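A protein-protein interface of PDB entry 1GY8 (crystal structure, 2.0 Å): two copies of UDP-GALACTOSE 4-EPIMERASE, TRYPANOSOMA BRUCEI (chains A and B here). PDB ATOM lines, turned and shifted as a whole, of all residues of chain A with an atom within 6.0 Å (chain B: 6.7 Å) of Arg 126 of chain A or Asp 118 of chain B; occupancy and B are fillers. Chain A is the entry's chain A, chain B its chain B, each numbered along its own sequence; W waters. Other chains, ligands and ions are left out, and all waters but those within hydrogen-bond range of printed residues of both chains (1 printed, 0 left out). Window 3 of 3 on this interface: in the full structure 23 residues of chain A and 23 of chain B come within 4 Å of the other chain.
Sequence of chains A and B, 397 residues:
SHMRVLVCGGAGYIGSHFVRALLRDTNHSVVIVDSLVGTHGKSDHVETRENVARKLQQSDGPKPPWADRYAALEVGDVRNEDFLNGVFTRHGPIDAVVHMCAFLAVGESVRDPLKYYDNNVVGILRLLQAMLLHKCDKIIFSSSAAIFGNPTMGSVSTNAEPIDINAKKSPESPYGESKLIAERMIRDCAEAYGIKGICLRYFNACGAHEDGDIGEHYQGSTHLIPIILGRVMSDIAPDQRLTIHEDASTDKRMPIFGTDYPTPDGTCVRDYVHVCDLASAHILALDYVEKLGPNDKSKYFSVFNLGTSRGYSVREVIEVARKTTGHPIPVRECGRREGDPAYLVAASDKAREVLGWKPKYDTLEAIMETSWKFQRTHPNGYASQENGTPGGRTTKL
The side-chain amide nitrogen of Gln 129 of chain A sits at hydrogen-bond distance from the side-chain carboxylate of Asp 118 of chain B, 2.9 Å away. OD2 of Asp 118 of chain B lies within salt-bridge range of NH1 of Arg 126 of chain A (3.0 Å).
OE1 of Glu 81 of chain A lies within salt-bridge range of NH1 of Arg 126 of chain A (3.8 Å). NH1 of Arg 126 of chain A is in hydrogen-bond range of OE1 of Gln 129 of chain A (2.9 Å). OD1 of Asp 118 of chain B lies within salt-bridge range of NH1 of Arg 79 of chain B, 2.8 Å away.
Leu 114 of chain B touches Leu 125 of chain A. Leu 125 of chain A touches Asp 118 of chain B. CD2 of Leu 125 of chain A touches CG2 of Val 122 of chain B (3.6 Å). Leu 114 of chain B touches Leu 128 of chain A (CD1 to O, 3.7 Å). Leu 114 of chain B touches Gln 129 of chain A.
Of the printed residues of chain B, Arg 126 of chain A touches Asp 118. Asp 118 of chain B touches just these residues of chain A: Leu 125, Arg 126 and Gln 129. Of the printed residues of chain B, Leu 125 of chain A touches Leu 114 (3.9 Å), Asp 118 (3.7 Å) and Val 122 (3.6 Å). Printed residues of chain A within 4 Å of Leu 114 of chain B: Leu 125 (3.9 Å), Leu 128 (3.7 Å) and Gln 129 (3.8 Å). Printed residues of chain B within 4 Å of Gln 129 of chain A: Leu 114 (3.8 Å) and Asp 118 (2.9 Å). Of the printed residues of chain A, Val 122 of chain B touches Leu 125 (3.6 Å). Glu 81 of chain A touches none of the printed residues of chain B. The nearest printed residue of chain B that does not touch Gln 129 of chain A is Lys 115 of chain B (5.5 Å).
Printed residues of chain B that touch a printed residue of chain A: Leu 114, Asp 118 and Val 122. Among the printed residues, 7 pairs touch across the chains. Among the printed residues, Asp or Glu carboxylates within 4 Å of a Lys or Arg side-chain nitrogen of the other chain: Arg 126 of chain A with Asp 118 of chain B.
Positions printed for both chains: 79, 121, 122, 123, 124 and 126.
Water W1 lies within hydrogen-bond range of OD1 of Asp 118 of chain B (2.6 Å) and NH2 of Arg 126 of chain A (2.9 Å).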
ATOM      1  N   VAL A  78     -22.213 -25.405 -20.558  1.00  0.00           N
ATOM      2  CA  VAL A  78     -21.854 -24.883 -19.234  1.00  0.00           C
ATOM      3  C   VAL A  78     -21.936 -25.950 -18.147  1.00  0.00           C
ATOM      4  O   VAL A  78     -21.439 -25.767 -17.035  1.00  0.00           O
ATOM      5  CB  VAL A  78     -22.731 -23.666 -18.821  1.00  0.00           C
ATOM      6  CG1 VAL A  78     -22.486 -22.511 -19.780  1.00  0.00           C
ATOM      7  CG2 VAL A  78     -24.207 -24.047 -18.803  1.00  0.00           C
ATOM      8  N   ARG A  79     -22.560 -27.073 -18.478  1.00  0.00           N
ATOM      9  CA  ARG A  79     -22.663 -28.176 -17.537  1.00  0.00           C
ATOM     10  C   ARG A  79     -21.397 -29.032 -17.584  1.00  0.00           C
ATOM     11  O   ARG A  79     -21.217 -29.917 -16.754  1.00  0.00           O
ATOM     12  CB  ARG A  79     -23.891 -29.030 -17.852  1.00  0.00           C
ATOM     13  CG  ARG A  79     -25.203 -28.333 -17.530  1.00  0.00           C
ATOM     14  CD  ARG A  79     -26.390 -29.136 -18.026  1.00  0.00           C
ATOM     15  NE  ARG A  79     -26.390 -29.237 -19.478  1.00  0.00           N
ATOM     16  CZ  ARG A  79     -27.333 -29.844 -20.193  1.00  0.00           C
ATOM     17  NH1 ARG A  79     -28.361 -30.416 -19.586  1.00  0.00           N
ATOM     18  NH2 ARG A  79     -27.262 -29.858 -21.519  1.00  0.00           N
ATOM     19  N   ASN A  80     -20.533 -28.767 -18.562  1.00  0.00           N
ATOM     20  CA  ASN A  80     -19.270 -29.487 -18.699  1.00  0.00           C
ATOM     21  C   ASN A  80     -18.296 -28.692 -17.827  1.00  0.00           C
ATOM     22  O   ASN A  80     -17.666 -27.725 -18.273  1.00  0.00           O
ATOM     23  CB  ASN A  80     -18.835 -29.508 -20.168  1.00  0.00           C
ATOM     24  CG  ASN A  80     -17.485 -30.178 -20.378  1.00  0.00           C
ATOM     25  OD1 ASN A  80     -17.115 -30.501 -21.508  1.00  0.00           O
ATOM     26  ND2 ASN A  80     -16.739 -30.373 -19.300  1.00  0.00           N
ATOM     27  N   GLU A  81     -18.262 -29.071 -16.551  1.00  0.00           N
ATOM     28  CA  GLU A  81     -17.445 -28.420 -15.532  1.00  0.00           C
ATOM     29  C   GLU A  81     -15.993 -28.174 -15.933  1.00  0.00           C
ATOM     30  O   GLU A  81     -15.420 -27.148 -15.586  1.00  0.00           O
ATOM     31  CB  GLU A  81     -17.546 -29.222 -14.224  1.00  0.00           C
ATOM     32  CG  GLU A  81     -19.009 -29.410 -13.773  1.00  0.00           C
ATOM     33  CD  GLU A  81     -19.185 -30.418 -12.639  1.00  0.00           C
ATOM     34  OE1 GLU A  81     -18.947 -30.060 -11.466  1.00  0.00           O
ATOM     35  OE2 GLU A  81     -19.561 -31.578 -12.926  1.00  0.00           O
ATOM     36  N   LEU A  84     -16.051 -25.359 -18.615  1.00  0.00           N
ATOM     37  CA  LEU A  84     -16.377 -24.122 -17.926  1.00  0.00           C
ATOM     38  C   LEU A  84     -15.189 -23.578 -17.134  1.00  0.00           C
ATOM     39  O   LEU A  84     -14.897 -22.379 -17.177  1.00  0.00           O
ATOM     40  CB  LEU A  84     -17.572 -24.340 -16.997  1.00  0.00           C
ATOM     41  CG  LEU A  84     -18.182 -23.081 -16.377  1.00  0.00           C
ATOM     42  CD1 LEU A  84     -18.650 -22.148 -17.484  1.00  0.00           C
ATOM     43  CD2 LEU A  84     -19.340 -23.463 -15.481  1.00  0.00           C
ATOM     44  N   VAL A 121     -31.727 -26.000 -14.435  1.00  0.00           N
ATOM     45  CA  VAL A 121     -31.293 -25.966 -13.043  1.00  0.00           C
ATOM     46  C   VAL A 121     -29.835 -26.369 -12.842  1.00  0.00           C
ATOM     47  O   VAL A 121     -29.125 -25.736 -12.062  1.00  0.00           O
ATOM     48  CB  VAL A 121     -32.200 -26.842 -12.154  1.00  0.00           C
ATOM     49  CG1 VAL A 121     -31.825 -26.660 -10.693  1.00  0.00           C
ATOM     50  CG2 VAL A 121     -33.657 -26.461 -12.363  1.00  0.00           C
ATOM     51  N   VAL A 122     -29.377 -27.409 -13.534  1.00  0.00           N
ATOM     52  CA  VAL A 122     -27.979 -27.827 -13.382  1.00  0.00           C
ATOM     53  C   VAL A 122     -27.054 -26.795 -14.032  1.00  0.00           C
ATOM     54  O   VAL A 122     -25.914 -26.608 -13.609  1.00  0.00           O
ATOM     55  CB  VAL A 122     -27.711 -29.230 -14.012  1.00  0.00           C
ATOM     56  CG1 VAL A 122     -26.244 -29.628 -13.815  1.00  0.00           C
ATOM     57  CG2 VAL A 122     -28.615 -30.274 -13.365  1.00  0.00           C
ATOM     58  N   GLY A 123     -27.553 -26.117 -15.058  1.00  0.00           N
ATOM     59  CA  GLY A 123     -26.753 -25.106 -15.723  1.00  0.00           C
ATOM     60  C   GLY A 123     -26.403 -23.941 -14.809  1.00  0.00           C
ATOM     61  O   GLY A 123     -25.250 -23.521 -14.754  1.00  0.00           O
ATOM     62  N   ILE A 124     -27.391 -23.414 -14.091  1.00  0.00           N
ATOM     63  CA  ILE A 124     -27.146 -22.300 -13.188  1.00  0.00           C
ATOM     64  C   ILE A 124     -26.344 -22.763 -11.965  1.00  0.00           C
ATOM     65  O   ILE A 124     -25.569 -21.996 -11.397  1.00  0.00           O
ATOM     66  CB  ILE A 124     -28.478 -21.625 -12.751  1.00  0.00           C
ATOM     67  CG1 ILE A 124     -28.187 -20.447 -11.815  1.00  0.00           C
ATOM     68  CG2 ILE A 124     -29.390 -22.637 -12.077  1.00  0.00           C
ATOM     69  CD1 ILE A 124     -27.347 -19.343 -12.442  1.00  0.00           C
ATOM     70  N   LEU A 125     -26.513 -24.025 -11.579  1.00  0.00           N
ATOM     71  CA  LEU A 125     -25.775 -24.576 -10.449  1.00  0.00           C
ATOM     72  C   LEU A 125     -24.274 -24.581 -10.757  1.00  0.00           C
ATOM     73  O   LEU A 125     -23.464 -24.175  -9.929  1.00  0.00           O
ATOM     74  CB  LEU A 125     -26.234 -26.007 -10.151  1.00  0.00           C
ATOM     75  CG  LEU A 125     -25.435 -26.801  -9.099  1.00  0.00           C
ATOM     76  CD1 LEU A 125     -25.688 -26.242  -7.701  1.00  0.00           C
ATOM     77  CD2 LEU A 125     -25.828 -28.274  -9.158  1.00  0.00           C
ATOM     78  N   ARG A 126     -23.913 -25.040 -11.951  1.00  0.00           N
ATOM     79  CA  ARG A 126     -22.516 -25.109 -12.353  1.00  0.00           C
ATOM     80  C   ARG A 126     -21.868 -23.734 -12.450  1.00  0.00           C
ATOM     81  O   ARG A 126     -20.700 -23.565 -12.087  1.00  0.00           O
ATOM     82  CB  ARG A 126     -22.382 -25.848 -13.686  1.00  0.00           C
ATOM     83  CG  ARG A 126     -22.904 -27.288 -13.660  1.00  0.00           C
ATOM     84  CD  ARG A 126     -22.370 -28.052 -12.455  1.00  0.00           C
ATOM     85  NE  ARG A 126     -22.790 -29.450 -12.471  1.00  0.00           N
ATOM     86  CZ  ARG A 126     -22.847 -30.230 -11.396  1.00  0.00           C
ATOM     87  NH1 ARG A 126     -22.512 -29.756 -10.205  1.00  0.00           N
ATOM     88  NH2 ARG A 126     -23.250 -31.488 -11.509  1.00  0.00           N
ATOM     89  N   LEU A 127     -22.619 -22.752 -12.942  1.00  0.00           N
ATOM     90  CA  LEU A 127     -22.097 -21.394 -13.042  1.00  0.00           C
ATOM     91  C   LEU A 127     -21.837 -20.821 -11.652  1.00  0.00           C
ATOM     92  O   LEU A 127     -20.785 -20.225 -11.404  1.00  0.00           O
ATOM     93  CB  LEU A 127     -23.071 -20.478 -13.798  1.00  0.00           C
ATOM     94  CG  LEU A 127     -22.679 -20.130 -15.236  1.00  0.00           C
ATOM     95  CD1 LEU A 127     -21.325 -19.414 -15.273  1.00  0.00           C
ATOM     96  CD2 LEU A 127     -22.609 -21.409 -16.055  1.00  0.00           C
ATOM     97  N   LEU A 128     -22.787 -21.015 -10.743  1.00  0.00           N
ATOM     98  CA  LEU A 128     -22.640 -20.506  -9.389  1.00  0.00           C
ATOM     99  C   LEU A 128     -21.446 -21.158  -8.706  1.00  0.00           C
ATOM    100  O   LEU A 128     -20.719 -20.498  -7.960  1.00  0.00           O
ATOM    101  CB  LEU A 128     -23.924 -20.737  -8.583  1.00  0.00           C
ATOM    102  CG  LEU A 128     -25.138 -19.887  -9.002  1.00  0.00           C
ATOM    103  CD1 LEU A 128     -26.397 -20.356  -8.280  1.00  0.00           C
ATOM    104  CD2 LEU A 128     -24.860 -18.421  -8.696  1.00  0.00           C
ATOM    105  N   GLN A 129     -21.235 -22.446  -8.969  1.00  0.00           N
ATOM    106  CA  GLN A 129     -20.105 -23.156  -8.378  1.00  0.00           C
ATOM    107  C   GLN A 129     -18.793 -22.634  -8.969  1.00  0.00           C
ATOM    108  O   GLN A 129     -17.806 -22.471  -8.252  1.00  0.00           O
ATOM    109  CB  GLN A 129     -20.250 -24.678  -8.593  1.00  0.00           C
ATOM    110  CG  GLN A 129     -21.442 -25.278  -7.830  1.00  0.00           C
ATOM    111  CD  GLN A 129     -21.676 -26.754  -8.107  1.00  0.00           C
ATOM    112  OE1 GLN A 129     -21.652 -27.197  -9.257  1.00  0.00           O
ATOM    113  NE2 GLN A 129     -21.928 -27.517  -7.050  1.00  0.00           N
ATOM    114  N   ALA A 130     -18.788 -22.351 -10.271  1.00  0.00           N
ATOM    115  CA  ALA A 130     -17.595 -21.832 -10.939  1.00  0.00           C
ATOM    116  C   ALA A 130     -17.266 -20.427 -10.440  1.00  0.00           C
ATOM    117  O   ALA A 130     -16.098 -20.086 -10.231  1.00  0.00           O
ATOM    118  CB  ALA A 130     -17.798 -21.813 -12.445  1.00  0.00           C
ATOM    119  N   MET A 131     -18.296 -19.609 -10.255  1.00  0.00           N
ATOM    120  CA  MET A 131     -18.101 -18.253  -9.763  1.00  0.00           C
ATOM    121  C   MET A 131     -17.424 -18.291  -8.395  1.00  0.00           C
ATOM    122  O   MET A 131     -16.520 -17.508  -8.116  1.00  0.00           O
ATOM    123  CB  MET A 131     -19.440 -17.531  -9.639  1.00  0.00           C
ATOM    124  CG  MET A 131     -20.093 -17.185 -10.946  1.00  0.00           C
ATOM    125  SD  MET A 131     -21.691 -16.413 -10.671  1.00  0.00           S
ATOM    126  CE  MET A 131     -21.216 -14.843  -9.903  1.00  0.00           C
ATOM    127  N   ARG B  79     -25.261 -39.665  -8.165  1.00  0.00           N
ATOM    128  CA  ARG B  79     -25.021 -38.645  -9.185  1.00  0.00           C
ATOM    129  C   ARG B  79     -24.032 -39.157 -10.232  1.00  0.00           C
ATOM    130  O   ARG B  79     -23.813 -38.515 -11.257  1.00  0.00           O
ATOM    131  CB  ARG B  79     -24.486 -37.363  -8.548  1.00  0.00           C
ATOM    132  CG  ARG B  79     -25.525 -36.612  -7.733  1.00  0.00           C
ATOM    133  CD  ARG B  79     -24.897 -35.456  -6.980  1.00  0.00           C
ATOM    134  NE  ARG B  79     -23.945 -35.929  -5.982  1.00  0.00           N
ATOM    135  CZ  ARG B  79     -23.286 -35.138  -5.142  1.00  0.00           C
ATOM    136  NH1 ARG B  79     -23.469 -33.826  -5.177  1.00  0.00           N
ATOM    137  NH2 ARG B  79     -22.452 -35.659  -4.253  1.00  0.00           N
ATOM    138  N   PHE B 103     -28.123 -34.366   1.985  1.00  0.00           N
ATOM    139  CA  PHE B 103     -27.381 -33.724   3.061  1.00  0.00           C
ATOM    140  C   PHE B 103     -28.544 -33.091   3.803  1.00  0.00           C
ATOM    141  O   PHE B 103     -29.463 -32.579   3.171  1.00  0.00           O
ATOM    142  CB  PHE B 103     -26.408 -32.672   2.520  1.00  0.00           C
ATOM    143  CG  PHE B 103     -25.183 -33.264   1.880  1.00  0.00           C
ATOM    144  CD1 PHE B 103     -24.545 -34.366   2.455  1.00  0.00           C
ATOM    145  CD2 PHE B 103     -24.668 -32.734   0.708  1.00  0.00           C
ATOM    146  CE1 PHE B 103     -23.408 -34.930   1.864  1.00  0.00           C
ATOM    147  CE2 PHE B 103     -23.537 -33.286   0.111  1.00  0.00           C
ATOM    148  CZ  PHE B 103     -22.905 -34.385   0.687  1.00  0.00           C
ATOM    149  N   PRO B 113     -25.256 -23.257   0.525  1.00  0.00           N
ATOM    150  CA  PRO B 113     -26.388 -23.622  -0.337  1.00  0.00           C
ATOM    151  C   PRO B 113     -26.055 -24.553  -1.504  1.00  0.00           C
ATOM    152  O   PRO B 113     -26.765 -25.533  -1.739  1.00  0.00           O
ATOM    153  CB  PRO B 113     -26.891 -22.268  -0.857  1.00  0.00           C
ATOM    154  CG  PRO B 113     -26.413 -21.292   0.137  1.00  0.00           C
ATOM    155  CD  PRO B 113     -25.053 -21.798   0.511  1.00  0.00           C
ATOM    156  N   LEU B 114     -24.988 -24.237  -2.238  1.00  0.00           N
ATOM    157  CA  LEU B 114     -24.612 -25.028  -3.407  1.00  0.00           C
ATOM    158  C   LEU B 114     -24.332 -26.498  -3.108  1.00  0.00           C
ATOM    159  O   LEU B 114     -24.562 -27.360  -3.955  1.00  0.00           O
ATOM    160  CB  LEU B 114     -23.417 -24.382  -4.121  1.00  0.00           C
ATOM    161  CG  LEU B 114     -23.682 -22.967  -4.662  1.00  0.00           C
ATOM    162  CD1 LEU B 114     -22.418 -22.424  -5.322  1.00  0.00           C
ATOM    163  CD2 LEU B 114     -24.850 -22.991  -5.660  1.00  0.00           C
ATOM    164  N   LYS B 115     -23.844 -26.784  -1.905  1.00  0.00           N
ATOM    165  CA  LYS B 115     -23.562 -28.159  -1.516  1.00  0.00           C
ATOM    166  C   LYS B 115     -24.881 -28.930  -1.432  1.00  0.00           C
ATOM    167  O   LYS B 115     -24.973 -30.104  -1.802  1.00  0.00           O
ATOM    168  CB  LYS B 115     -22.856 -28.189  -0.161  1.00  0.00           C
ATOM    169  CG  LYS B 115     -22.623 -29.597   0.389  1.00  0.00           C
ATOM    170  CD  LYS B 115     -21.882 -29.554   1.716  1.00  0.00           C
ATOM    171  CE  LYS B 115     -21.700 -30.947   2.297  1.00  0.00           C
ATOM    172  NZ  LYS B 115     -20.945 -30.920   3.579  1.00  0.00           N
ATOM    173  N   TYR B 116     -25.907 -28.247  -0.945  1.00  0.00           N
ATOM    174  CA  TYR B 116     -27.228 -28.836  -0.805  1.00  0.00           C
ATOM    175  C   TYR B 116     -28.027 -28.885  -2.095  1.00  0.00           C
ATOM    176  O   TYR B 116     -28.703 -29.878  -2.361  1.00  0.00           O
ATOM    177  CB  TYR B 116     -28.010 -28.102   0.284  1.00  0.00           C
ATOM    178  CG  TYR B 116     -27.604 -28.541   1.667  1.00  0.00           C
ATOM    179  CD1 TYR B 116     -26.320 -28.273   2.154  1.00  0.00           C
ATOM    180  CD2 TYR B 116     -28.465 -29.304   2.457  1.00  0.00           C
ATOM    181  CE1 TYR B 116     -25.903 -28.759   3.376  1.00  0.00           C
ATOM    182  CE2 TYR B 116     -28.055 -29.797   3.692  1.00  0.00           C
ATOM    183  CZ  TYR B 116     -26.772 -29.525   4.141  1.00  0.00           C
ATOM    184  OH  TYR B 116     -26.346 -30.049   5.331  1.00  0.00           O
ATOM    185  N   TYR B 117     -27.969 -27.829  -2.896  1.00  0.00           N
ATOM    186  CA  TYR B 117     -28.699 -27.836  -4.152  1.00  0.00           C
ATOM    187  C   TYR B 117     -28.102 -28.902  -5.063  1.00  0.00           C
ATOM    188  O   TYR B 117     -28.828 -29.616  -5.751  1.00  0.00           O
ATOM    189  CB  TYR B 117     -28.644 -26.459  -4.820  1.00  0.00           C
ATOM    190  CG  TYR B 117     -29.613 -25.463  -4.215  1.00  0.00           C
ATOM    191  CD1 TYR B 117     -30.988 -25.668  -4.291  1.00  0.00           C
ATOM    192  CD2 TYR B 117     -29.153 -24.317  -3.560  1.00  0.00           C
ATOM    193  CE1 TYR B 117     -31.889 -24.756  -3.732  1.00  0.00           C
ATOM    194  CE2 TYR B 117     -30.044 -23.400  -3.000  1.00  0.00           C
ATOM    195  CZ  TYR B 117     -31.410 -23.625  -3.092  1.00  0.00           C
ATOM    196  OH  TYR B 117     -32.292 -22.712  -2.557  1.00  0.00           O
ATOM    197  N   ASP B 118     -26.782 -29.031  -5.046  1.00  0.00           N
ATOM    198  CA  ASP B 118     -26.125 -30.021  -5.883  1.00  0.00           C
ATOM    199  C   ASP B 118     -26.553 -31.439  -5.493  1.00  0.00           C
ATOM    200  O   ASP B 118     -27.214 -32.139  -6.265  1.00  0.00           O
ATOM    201  CB  ASP B 118     -24.603 -29.899  -5.755  1.00  0.00           C
ATOM    202  CG  ASP B 118     -23.859 -30.762  -6.754  1.00  0.00           C
ATOM    203  OD1 ASP B 118     -24.289 -31.904  -6.999  1.00  0.00           O
ATOM    204  OD2 ASP B 118     -22.829 -30.307  -7.289  1.00  0.00           O
ATOM    205  N   ASN B 119     -26.190 -31.858  -4.287  1.00  0.00           N
ATOM    206  CA  ASN B 119     -26.519 -33.205  -3.851  1.00  0.00           C
ATOM    207  C   ASN B 119     -28.007 -33.513  -3.797  1.00  0.00           C
ATOM    208  O   ASN B 119     -28.458 -34.529  -4.325  1.00  0.00           O
ATOM    209  CB  ASN B 119     -25.897 -33.492  -2.482  1.00  0.00           C
ATOM    210  CG  ASN B 119     -25.920 -34.972  -2.140  1.00  0.00           C
ATOM    211  OD1 ASN B 119     -25.656 -35.809  -2.996  1.00  0.00           O
ATOM    212  ND2 ASN B 119     -26.222 -35.299  -0.895  1.00  0.00           N
ATOM    213  N   ASN B 120     -28.774 -32.636  -3.170  1.00  0.00           N
ATOM    214  CA  ASN B 120     -30.200 -32.875  -3.032  1.00  0.00           C
ATOM    215  C   ASN B 120     -31.018 -32.782  -4.308  1.00  0.00           C
ATOM    216  O   ASN B 120     -31.873 -33.636  -4.545  1.00  0.00           O
ATOM    217  CB  ASN B 120     -30.769 -31.950  -1.957  1.00  0.00           C
ATOM    218  CG  ASN B 120     -30.187 -32.243  -0.581  1.00  0.00           C
ATOM    219  OD1 ASN B 120     -29.218 -32.993  -0.457  1.00  0.00           O
ATOM    220  ND2 ASN B 120     -30.766 -31.653   0.451  1.00  0.00           N
ATOM    221  N   VAL B 121     -30.763 -31.770  -5.135  1.00  0.00           N
ATOM    222  CA  VAL B 121     -31.526 -31.615  -6.363  1.00  0.00           C
ATOM    223  C   VAL B 121     -30.990 -32.435  -7.530  1.00  0.00           C
ATOM    224  O   VAL B 121     -31.767 -33.024  -8.273  1.00  0.00           O
ATOM    225  CB  VAL B 121     -31.630 -30.126  -6.777  1.00  0.00           C
ATOM    226  CG1 VAL B 121     -32.564 -29.976  -7.966  1.00  0.00           C
ATOM    227  CG2 VAL B 121     -32.149 -29.302  -5.602  1.00  0.00           C
ATOM    228  N   VAL B 122     -29.673 -32.485  -7.702  1.00  0.00           N
ATOM    229  CA  VAL B 122     -29.116 -33.266  -8.806  1.00  0.00           C
ATOM    230  C   VAL B 122     -29.275 -34.754  -8.511  1.00  0.00           C
ATOM    231  O   VAL B 122     -29.405 -35.562  -9.426  1.00  0.00           O
ATOM    232  CB  VAL B 122     -27.611 -32.948  -9.055  1.00  0.00           C
ATOM    233  CG1 VAL B 122     -27.084 -33.780 -10.226  1.00  0.00           C
ATOM    234  CG2 VAL B 122     -27.427 -31.459  -9.359  1.00  0.00           C
ATOM    235  N   GLY B 123     -29.275 -35.110  -7.231  1.00  0.00           N
ATOM    236  CA  GLY B 123     -29.439 -36.504  -6.858  1.00  0.00           C
ATOM    237  C   GLY B 123     -30.790 -37.066  -7.275  1.00  0.00           C
ATOM    238  O   GLY B 123     -30.859 -38.146  -7.853  1.00  0.00           O
ATOM    239  N   ILE B 124     -31.868 -36.340  -6.988  1.00  0.00           N
ATOM    240  CA  ILE B 124     -33.200 -36.802  -7.355  1.00  0.00           C
ATOM    241  C   ILE B 124     -33.402 -36.727  -8.873  1.00  0.00           C
ATOM    242  O   ILE B 124     -34.143 -37.524  -9.450  1.00  0.00           O
ATOM    243  CB  ILE B 124     -34.301 -35.988  -6.617  1.00  0.00           C
ATOM    244  CG1 ILE B 124     -35.690 -36.511  -6.999  1.00  0.00           C
ATOM    245  CG2 ILE B 124     -34.169 -34.509  -6.937  1.00  0.00           C
ATOM    246  CD1 ILE B 124     -35.930 -37.973  -6.628  1.00  0.00           C
ATOM    247  N   ARG B 126     -31.093 -37.345 -11.196  1.00  0.00           N
ATOM    248  CA  ARG B 126     -30.457 -38.525 -11.779  1.00  0.00           C
ATOM    249  C   ARG B 126     -31.284 -39.789 -11.582  1.00  0.00           C
ATOM    250  O   ARG B 126     -31.355 -40.631 -12.474  1.00  0.00           O
ATOM    251  CB  ARG B 126     -29.056 -38.716 -11.193  1.00  0.00           C
ATOM    252  CG  ARG B 126     -28.110 -37.548 -11.446  1.00  0.00           C
ATOM    253  CD  ARG B 126     -28.145 -37.103 -12.906  1.00  0.00           C
ATOM    254  NE  ARG B 126     -27.189 -36.031 -13.170  1.00  0.00           N
ATOM    255  CZ  ARG B 126     -27.270 -35.179 -14.190  1.00  0.00           C
ATOM    256  NH1 ARG B 126     -28.267 -35.263 -15.053  1.00  0.00           N
ATOM    257  NH2 ARG B 126     -26.348 -34.237 -14.350  1.00  0.00           N
HETATM  258  O   HOH W   1     -23.201 -33.039  -9.064  1.00  0.00           O
